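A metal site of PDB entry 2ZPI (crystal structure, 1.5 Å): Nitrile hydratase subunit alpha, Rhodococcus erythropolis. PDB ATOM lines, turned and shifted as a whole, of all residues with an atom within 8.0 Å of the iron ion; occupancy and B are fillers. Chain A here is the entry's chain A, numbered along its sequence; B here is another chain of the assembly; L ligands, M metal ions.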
ATOM      1  N   GLN A  90      -7.753  25.992  28.135  1.00  0.00           N
ATOM      2  CA  GLN A  90      -7.647  25.370  26.813  1.00  0.00           C
ATOM      3  C   GLN A  90      -8.785  24.381  26.570  1.00  0.00           C
ATOM      4  O   GLN A  90      -8.650  23.387  25.848  1.00  0.00           O
ATOM      5  CB  GLN A  90      -6.265  24.710  26.630  1.00  0.00           C
ATOM      6  CG  GLN A  90      -5.126  25.728  26.607  1.00  0.00           C
ATOM      7  CD  GLN A  90      -5.285  26.728  25.492  1.00  0.00           C
ATOM      8  OE1 GLN A  90      -5.336  26.352  24.319  1.00  0.00           O
ATOM      9  NE2 GLN A  90      -5.404  28.013  25.834  1.00  0.00           N
ATOM     10  N   VAL A 108      -5.794  17.998  14.874  1.00  0.00           N
ATOM     11  CA  VAL A 108      -4.383  18.401  14.956  1.00  0.00           C
ATOM     12  C   VAL A 108      -4.322  19.892  15.314  1.00  0.00           C
ATOM     13  O   VAL A 108      -5.328  20.596  15.216  1.00  0.00           O
ATOM     14  CB  VAL A 108      -3.661  18.147  13.604  1.00  0.00           C
ATOM     15  CG1 VAL A 108      -4.263  19.016  12.497  1.00  0.00           C
ATOM     16  CG2 VAL A 108      -2.161  18.407  13.721  1.00  0.00           C
ATOM     17  N   CYS A 109      -3.164  20.355  15.763  1.00  0.00           N
ATOM     18  CA  CYS A 109      -2.841  21.777  15.739  1.00  0.00           C
ATOM     19  C   CYS A 109      -1.579  21.955  14.904  1.00  0.00           C
ATOM     20  O   CYS A 109      -0.464  21.765  15.391  1.00  0.00           O
ATOM     21  CB  CYS A 109      -2.595  22.308  17.151  1.00  0.00           C
ATOM     22  SG  CYS A 109      -2.148  24.068  17.147  1.00  0.00           S
ATOM     23  N   SER A 110      -1.734  22.270  13.625  1.00  0.00           N
ATOM     24  CA  SER A 110      -0.567  22.296  12.764  1.00  0.00           C
ATOM     25  C   SER A 110       0.402  23.428  13.148  1.00  0.00           C
ATOM     26  O   SER A 110       1.610  23.313  12.921  1.00  0.00           O
ATOM     27  CB  SER A 110      -0.954  22.416  11.288  1.00  0.00           C
ATOM     28  OG  SER A 110      -1.522  23.685  11.027  1.00  0.00           O
ATOM     29  N   LEU A 111      -0.124  24.484  13.764  1.00  0.00           N
ATOM     30  CA  LEU A 111       0.678  25.676  14.067  1.00  0.00           C
ATOM     31  C   LEU A 111       1.429  25.580  15.398  1.00  0.00           C
ATOM     32  O   LEU A 111       2.331  26.387  15.669  1.00  0.00           O
ATOM     33  CB  LEU A 111      -0.211  26.923  14.067  1.00  0.00           C
ATOM     34  CG  LEU A 111      -0.800  27.257  12.695  1.00  0.00           C
ATOM     35  CD1 LEU A 111      -1.864  28.326  12.847  1.00  0.00           C
ATOM     36  CD2 LEU A 111       0.279  27.718  11.711  1.00  0.00           C
ATOM     37  N   CSD A 112       1.016  24.556  16.382  1.00  0.00           N
ATOM     38  CA  CSD A 112       1.686  24.475  17.669  1.00  0.00           C
ATOM     39  CB  CSD A 112       1.419  25.720  18.527  1.00  0.00           C
ATOM     40  SG  CSD A 112      -0.259  26.282  18.639  1.00  0.00           S
ATOM     41  C   CSD A 112       1.221  23.200  18.346  1.00  0.00           C
ATOM     42  O   CSD A 112       1.833  22.146  18.185  1.00  0.00           O
ATOM     43  OD1 CSD A 112      -0.178  27.351  19.714  1.00  0.00           O
ATOM     44  OD2 CSD A 112      -0.620  26.854  17.291  1.00  0.00           O
ATOM     45  N   SER A 113       0.052  23.223  19.202  1.00  0.00           N
ATOM     46  CA  SER A 113      -0.225  21.951  19.932  1.00  0.00           C
ATOM     47  C   SER A 113      -1.639  21.957  20.500  1.00  0.00           C
ATOM     48  O   SER A 113      -2.030  21.032  21.212  1.00  0.00           O
ATOM     49  CB  SER A 113       0.788  21.762  21.066  1.00  0.00           C
ATOM     50  OG  SER A 113       0.674  22.822  22.008  1.00  0.00           O
ATOM     51  N   CSO A 114      -2.398  23.016  20.036  1.00  0.00           N
ATOM     52  CA  CSO A 114      -3.708  23.290  20.629  1.00  0.00           C
ATOM     53  CB  CSO A 114      -4.412  24.351  19.789  1.00  0.00           C
ATOM     54  SG  CSO A 114      -3.278  25.717  19.601  1.00  0.00           S
ATOM     55  C   CSO A 114      -4.526  22.017  20.681  1.00  0.00           C
ATOM     56  O   CSO A 114      -4.681  21.234  19.739  1.00  0.00           O
ATOM     57  OD  CSO A 114      -3.288  26.381  20.993  1.00  0.00           O
ATOM     58  N   THR A 115      -5.067  21.786  21.952  1.00  0.00           N
ATOM     59  CA  THR A 115      -5.689  20.528  22.448  1.00  0.00           C
ATOM     60  C   THR A 115      -6.697  20.892  23.527  1.00  0.00           C
ATOM     61  O   THR A 115      -6.454  21.805  24.295  1.00  0.00           O
ATOM     62  CB  THR A 115      -4.618  19.614  23.068  1.00  0.00           C
ATOM     63  OG1 THR A 115      -3.742  19.160  22.021  1.00  0.00           O
ATOM     64  CG2 THR A 115      -5.234  18.403  23.762  1.00  0.00           C
ATOM     65  N   TRP A 117      -7.320  20.418  26.577  1.00  0.00           N
ATOM     66  CA  TRP A 117      -6.603  19.879  27.743  1.00  0.00           C
ATOM     67  C   TRP A 117      -7.468  19.197  28.817  1.00  0.00           C
ATOM     68  O   TRP A 117      -7.135  18.114  29.272  1.00  0.00           O
ATOM     69  CB  TRP A 117      -5.820  20.972  28.463  1.00  0.00           C
ATOM     70  CG  TRP A 117      -4.633  21.529  27.744  1.00  0.00           C
ATOM     71  CD1 TRP A 117      -4.049  21.077  26.605  1.00  0.00           C
ATOM     72  CD2 TRP A 117      -3.884  22.654  28.176  1.00  0.00           C
ATOM     73  NE1 TRP A 117      -2.959  21.859  26.294  1.00  0.00           N
ATOM     74  CE2 TRP A 117      -2.842  22.839  27.249  1.00  0.00           C
ATOM     75  CE3 TRP A 117      -3.975  23.524  29.275  1.00  0.00           C
ATOM     76  CZ2 TRP A 117      -1.914  23.883  27.376  1.00  0.00           C
ATOM     77  CZ3 TRP A 117      -3.060  24.549  29.393  1.00  0.00           C
ATOM     78  CH2 TRP A 117      -2.032  24.716  28.457  1.00  0.00           C
ATOM     79  N   PRO A 123      -1.394  17.407  25.429  1.00  0.00           N
ATOM     80  CA  PRO A 123      -1.038  16.648  24.231  1.00  0.00           C
ATOM     81  C   PRO A 123       0.226  15.836  24.441  1.00  0.00           C
ATOM     82  O   PRO A 123       1.139  16.264  25.149  1.00  0.00           O
ATOM     83  CB  PRO A 123      -0.814  17.737  23.177  1.00  0.00           C
ATOM     84  CG  PRO A 123      -0.501  18.971  23.957  1.00  0.00           C
ATOM     85  CD  PRO A 123      -1.352  18.856  25.200  1.00  0.00           C
ATOM     86  N   TYR A 127       1.857  14.139  19.150  1.00  0.00           N
ATOM     87  CA  TYR A 127       0.839  15.020  18.581  1.00  0.00           C
ATOM     88  C   TYR A 127       1.470  16.377  18.304  1.00  0.00           C
ATOM     89  O   TYR A 127       1.073  17.092  17.383  1.00  0.00           O
ATOM     90  CB  TYR A 127      -0.313  15.135  19.560  1.00  0.00           C
ATOM     91  CG  TYR A 127      -1.431  16.114  19.226  1.00  0.00           C
ATOM     92  CD1 TYR A 127      -1.346  17.460  19.597  1.00  0.00           C
ATOM     93  CD2 TYR A 127      -2.586  15.683  18.576  1.00  0.00           C
ATOM     94  CE1 TYR A 127      -2.382  18.344  19.329  1.00  0.00           C
ATOM     95  CE2 TYR A 127      -3.628  16.547  18.306  1.00  0.00           C
ATOM     96  CZ  TYR A 127      -3.523  17.881  18.681  1.00  0.00           C
ATOM     97  OH  TYR A 127      -4.581  18.752  18.449  1.00  0.00           O
ATOM     98  N   LYS A 128       2.449  16.724  19.139  1.00  0.00           N
ATOM     99  CA  LYS A 128       3.190  17.976  19.004  1.00  0.00           C
ATOM    100  C   LYS A 128       4.362  17.863  18.035  1.00  0.00           C
ATOM    101  O   LYS A 128       5.048  18.850  17.769  1.00  0.00           O
ATOM    102  CB  LYS A 128       3.699  18.419  20.385  1.00  0.00           C
ATOM    103  CG  LYS A 128       2.590  18.554  21.404  1.00  0.00           C
ATOM    104  CD  LYS A 128       3.144  18.890  22.760  1.00  0.00           C
ATOM    105  CE  LYS A 128       3.661  17.661  23.477  1.00  0.00           C
ATOM    106  NZ  LYS A 128       3.746  17.899  24.952  1.00  0.00           N
ATOM    107  N   ARG A 133       2.194  17.352  12.776  1.00  0.00           N
ATOM    108  CA  ARG A 133       1.800  18.712  12.402  1.00  0.00           C
ATOM    109  C   ARG A 133       1.893  18.970  10.895  1.00  0.00           C
ATOM    110  O   ARG A 133       1.025  19.619  10.308  1.00  0.00           O
ATOM    111  CB  ARG A 133       2.632  19.722  13.202  1.00  0.00           C
ATOM    112  CG  ARG A 133       2.249  19.751  14.692  1.00  0.00           C
ATOM    113  CD  ARG A 133       3.115  20.707  15.505  1.00  0.00           C
ATOM    114  NE  ARG A 133       3.226  21.988  14.831  1.00  0.00           N
ATOM    115  CZ  ARG A 133       4.198  22.872  15.056  1.00  0.00           C
ATOM    116  NH1 ARG A 133       5.133  22.637  15.964  1.00  0.00           N
ATOM    117  NH2 ARG A 133       4.242  23.993  14.349  1.00  0.00           N
ATOM    118  N   ASP A 161      -8.100  21.310  11.995  1.00  0.00           N
ATOM    119  CA  ASP A 161      -6.893  22.009  12.404  1.00  0.00           C
ATOM    120  C   ASP A 161      -7.299  23.047  13.440  1.00  0.00           C
ATOM    121  O   ASP A 161      -8.086  23.964  13.153  1.00  0.00           O
ATOM    122  CB  ASP A 161      -6.228  22.660  11.194  1.00  0.00           C
ATOM    123  CG  ASP A 161      -4.786  23.051  11.445  1.00  0.00           C
ATOM    124  OD1 ASP A 161      -4.347  22.978  12.621  1.00  0.00           O
ATOM    125  OD2 ASP A 161      -4.103  23.424  10.469  1.00  0.00           O
ATOM    126  N   THR A 162      -6.751  22.902  14.645  1.00  0.00           N
ATOM    127  CA  THR A 162      -7.152  23.721  15.780  1.00  0.00           C
ATOM    128  C   THR A 162      -6.412  25.039  15.761  1.00  0.00           C
ATOM    129  O   THR A 162      -5.391  25.216  16.412  1.00  0.00           O
ATOM    130  CB  THR A 162      -6.891  22.965  17.106  1.00  0.00           C
ATOM    131  OG1 THR A 162      -7.465  21.649  17.024  1.00  0.00           O
ATOM    132  CG2 THR A 162      -7.499  23.708  18.286  1.00  0.00           C
ATOM    133  N   THR A 163      -6.940  25.981  14.979  1.00  0.00           N
ATOM    134  CA  THR A 163      -6.252  27.223  14.675  1.00  0.00           C
ATOM    135  C   THR A 163      -6.739  28.432  15.467  1.00  0.00           C
ATOM    136  O   THR A 163      -6.126  29.502  15.396  1.00  0.00           O
ATOM    137  CB  THR A 163      -6.365  27.541  13.182  1.00  0.00           C
ATOM    138  OG1 THR A 163      -7.742  27.384  12.772  1.00  0.00           O
ATOM    139  CG2 THR A 163      -5.482  26.587  12.369  1.00  0.00           C
ATOM    140  N   ALA A 164      -7.825  28.278  16.218  1.00  0.00           N
ATOM    141  CA  ALA A 164      -8.343  29.400  17.020  1.00  0.00           C
ATOM    142  C   ALA A 164      -8.701  28.955  18.424  1.00  0.00           C
ATOM    143  O   ALA A 164      -7.881  28.302  19.065  1.00  0.00           O
ATOM    144  CB  ALA A 164      -9.520  30.093  16.318  1.00  0.00           C
ATOM    145  N   ARG A 167     -11.969  24.093  20.822  1.00  0.00           N
ATOM    146  CA  ARG A 167     -11.195  22.939  21.236  1.00  0.00           C
ATOM    147  C   ARG A 167     -12.058  21.724  20.978  1.00  0.00           C
ATOM    148  O   ARG A 167     -13.222  21.676  21.383  1.00  0.00           O
ATOM    149  CB  ARG A 167     -10.810  23.074  22.711  1.00  0.00           C
ATOM    150  CG  ARG A 167      -9.846  24.224  22.963  1.00  0.00           C
ATOM    151  CD  ARG A 167      -8.442  23.903  22.414  1.00  0.00           C
ATOM    152  NE  ARG A 167      -7.544  25.048  22.580  1.00  0.00           N
ATOM    153  CZ  ARG A 167      -7.429  26.042  21.691  1.00  0.00           C
ATOM    154  NH1 ARG A 167      -8.142  26.023  20.571  1.00  0.00           N
ATOM    155  NH2 ARG A 167      -6.606  27.047  21.926  1.00  0.00           N
ATOM    156  N   TYR B  37       4.375  26.065  31.049  1.00  0.00           N
ATOM    157  CA  TYR B  37       2.943  26.368  31.082  1.00  0.00           C
ATOM    158  C   TYR B  37       2.552  27.110  32.363  1.00  0.00           C
ATOM    159  O   TYR B  37       1.764  28.066  32.325  1.00  0.00           O
ATOM    160  CB  TYR B  37       2.068  25.104  30.978  1.00  0.00           C
ATOM    161  CG  TYR B  37       1.954  24.428  29.614  1.00  0.00           C
ATOM    162  CD1 TYR B  37       2.428  25.015  28.438  1.00  0.00           C
ATOM    163  CD2 TYR B  37       1.309  23.202  29.514  1.00  0.00           C
ATOM    164  CE1 TYR B  37       2.285  24.358  27.216  1.00  0.00           C
ATOM    165  CE2 TYR B  37       1.154  22.559  28.316  1.00  0.00           C
ATOM    166  CZ  TYR B  37       1.635  23.138  27.175  1.00  0.00           C
ATOM    167  OH  TYR B  37       1.453  22.453  25.987  1.00  0.00           O
ATOM    168  N   ARG B  56       2.235  32.375  21.764  1.00  0.00           N
ATOM    169  CA  ARG B  56       2.332  31.694  20.473  1.00  0.00           C
ATOM    170  C   ARG B  56       3.292  32.451  19.551  1.00  0.00           C
ATOM    171  O   ARG B  56       4.150  31.854  18.897  1.00  0.00           O
ATOM    172  CB  ARG B  56       0.957  31.591  19.808  1.00  0.00           C
ATOM    173  CG  ARG B  56      -0.031  30.710  20.554  1.00  0.00           C
ATOM    174  CD  ARG B  56      -1.216  30.327  19.687  1.00  0.00           C
ATOM    175  NE  ARG B  56      -2.085  29.465  20.464  1.00  0.00           N
ATOM    176  CZ  ARG B  56      -3.082  29.910  21.224  1.00  0.00           C
ATOM    177  NH1 ARG B  56      -3.380  31.205  21.260  1.00  0.00           N
ATOM    178  NH2 ARG B  56      -3.805  29.049  21.941  1.00  0.00           N
ATOM    179  N   TYR B  72       9.588  20.533  22.193  1.00  0.00           N
ATOM    180  CA  TYR B  72       8.396  21.313  22.503  1.00  0.00           C
ATOM    181  C   TYR B  72       8.457  22.157  23.785  1.00  0.00           C
ATOM    182  O   TYR B  72       8.330  23.382  23.727  1.00  0.00           O
ATOM    183  CB  TYR B  72       7.163  20.407  22.547  1.00  0.00           C
ATOM    184  CG  TYR B  72       5.892  21.155  22.870  1.00  0.00           C
ATOM    185  CD1 TYR B  72       5.149  21.751  21.863  1.00  0.00           C
ATOM    186  CD2 TYR B  72       5.480  21.303  24.191  1.00  0.00           C
ATOM    187  CE1 TYR B  72       4.003  22.449  22.158  1.00  0.00           C
ATOM    188  CE2 TYR B  72       4.343  22.011  24.498  1.00  0.00           C
ATOM    189  CZ  TYR B  72       3.615  22.582  23.476  1.00  0.00           C
ATOM    190  OH  TYR B  72       2.464  23.290  23.749  1.00  0.00           O
ATOM    191  N   TYR B  76       8.819  26.729  24.889  1.00  0.00           N
ATOM    192  CA  TYR B  76       7.986  27.581  25.755  1.00  0.00           C
ATOM    193  C   TYR B  76       8.770  28.161  26.923  1.00  0.00           C
ATOM    194  O   TYR B  76       8.464  29.262  27.363  1.00  0.00           O
ATOM    195  CB  TYR B  76       6.685  26.848  26.163  1.00  0.00           C
ATOM    196  CG  TYR B  76       5.847  26.624  24.927  1.00  0.00           C
ATOM    197  CD1 TYR B  76       4.894  27.557  24.534  1.00  0.00           C
ATOM    198  CD2 TYR B  76       6.091  25.546  24.097  1.00  0.00           C
ATOM    199  CE1 TYR B  76       4.160  27.390  23.348  1.00  0.00           C
ATOM    200  CE2 TYR B  76       5.379  25.370  22.930  1.00  0.00           C
ATOM    201  CZ  TYR B  76       4.409  26.284  22.565  1.00  0.00           C
ATOM    202  OH  TYR B  76       3.729  26.083  21.379  1.00  0.00           O
ATOM    203  N   ARG B 141      -3.433  33.640  12.720  1.00  0.00           N
ATOM    204  CA  ARG B 141      -3.886  32.265  12.940  1.00  0.00           C
ATOM    205  C   ARG B 141      -4.502  31.688  11.670  1.00  0.00           C
ATOM    206  O   ARG B 141      -5.547  31.020  11.689  1.00  0.00           O
ATOM    207  CB  ARG B 141      -4.851  32.196  14.128  1.00  0.00           C
ATOM    208  CG  ARG B 141      -4.161  32.530  15.433  1.00  0.00           C
ATOM    209  CD  ARG B 141      -2.976  31.580  15.670  1.00  0.00           C
ATOM    210  NE  ARG B 141      -3.410  30.223  15.956  1.00  0.00           N
ATOM    211  CZ  ARG B 141      -2.584  29.229  16.274  1.00  0.00           C
ATOM    212  NH1 ARG B 141      -1.275  29.431  16.264  1.00  0.00           N
ATOM    213  NH2 ARG B 141      -3.075  28.037  16.596  1.00  0.00           N
HETATM  214  C1  LIG L   1      -0.759  25.055  21.216  1.00  0.00           C
HETATM  215  N1  LIG L   1      -0.548  25.993  22.906  1.00  0.00           N
HETATM  216  C2  LIG L   1      -0.343  26.854  24.039  1.00  0.00           C
HETATM  217  C3  LIG L   1      -1.640  26.926  24.777  1.00  0.00           C
HETATM  218  C4  LIG L   1      -0.110  28.229  23.560  1.00  0.00           C
HETATM  219  C5  LIG L   1       0.827  26.446  24.940  1.00  0.00           C
HETATM  220 FE    FE M   1      -1.434  24.560  19.272  1.00  0.00          FE
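O of CSO 114 sits at hydrogen-bond distance from the side-chain hydroxyl of Tyr 127 (2.8 Å).
The side-chain sulfur of Cys 109 lies close to the backbone carbonyl oxygen of Thr 162 (3.5 Å).
The side-chain hydroxyl (OH) of Tyr 72 of chain B lies within hydrogen-bond range of the side-chain hydroxyl (OG) of Ser 113, at 2.5 Å.
The backbone NH (N) of Cys 109 sits at hydrogen-bond distance from the side-chain hydroxyl (OH) of Tyr 127.
The guanidinium group (NH2) of Arg 141 of chain B lies within salt-bridge range of OD2 of CSD 112, 2.8 Å away.
The backbone carbonyl oxygen of Ser 113 sits at hydrogen-bond distance from the side-chain hydroxyl of Thr 115.
NE of Arg 56 of chain B is in salt-bridge range of OD1 of CSD 112 (2.9 Å).
The guanidinium group (NH2) of Arg 56 of chain B sits at hydrogen-bond distance from OD of CSO 114.
Of the 24 residues printed, 4 come within 4 Å of the iron ion.
The iron ion is bound by N of CSO 114, N of Ser 113, SG of CSD 112, SG of CSO 114 and SG of Cys 109.
The iron ion has five donor atoms within binding distance.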
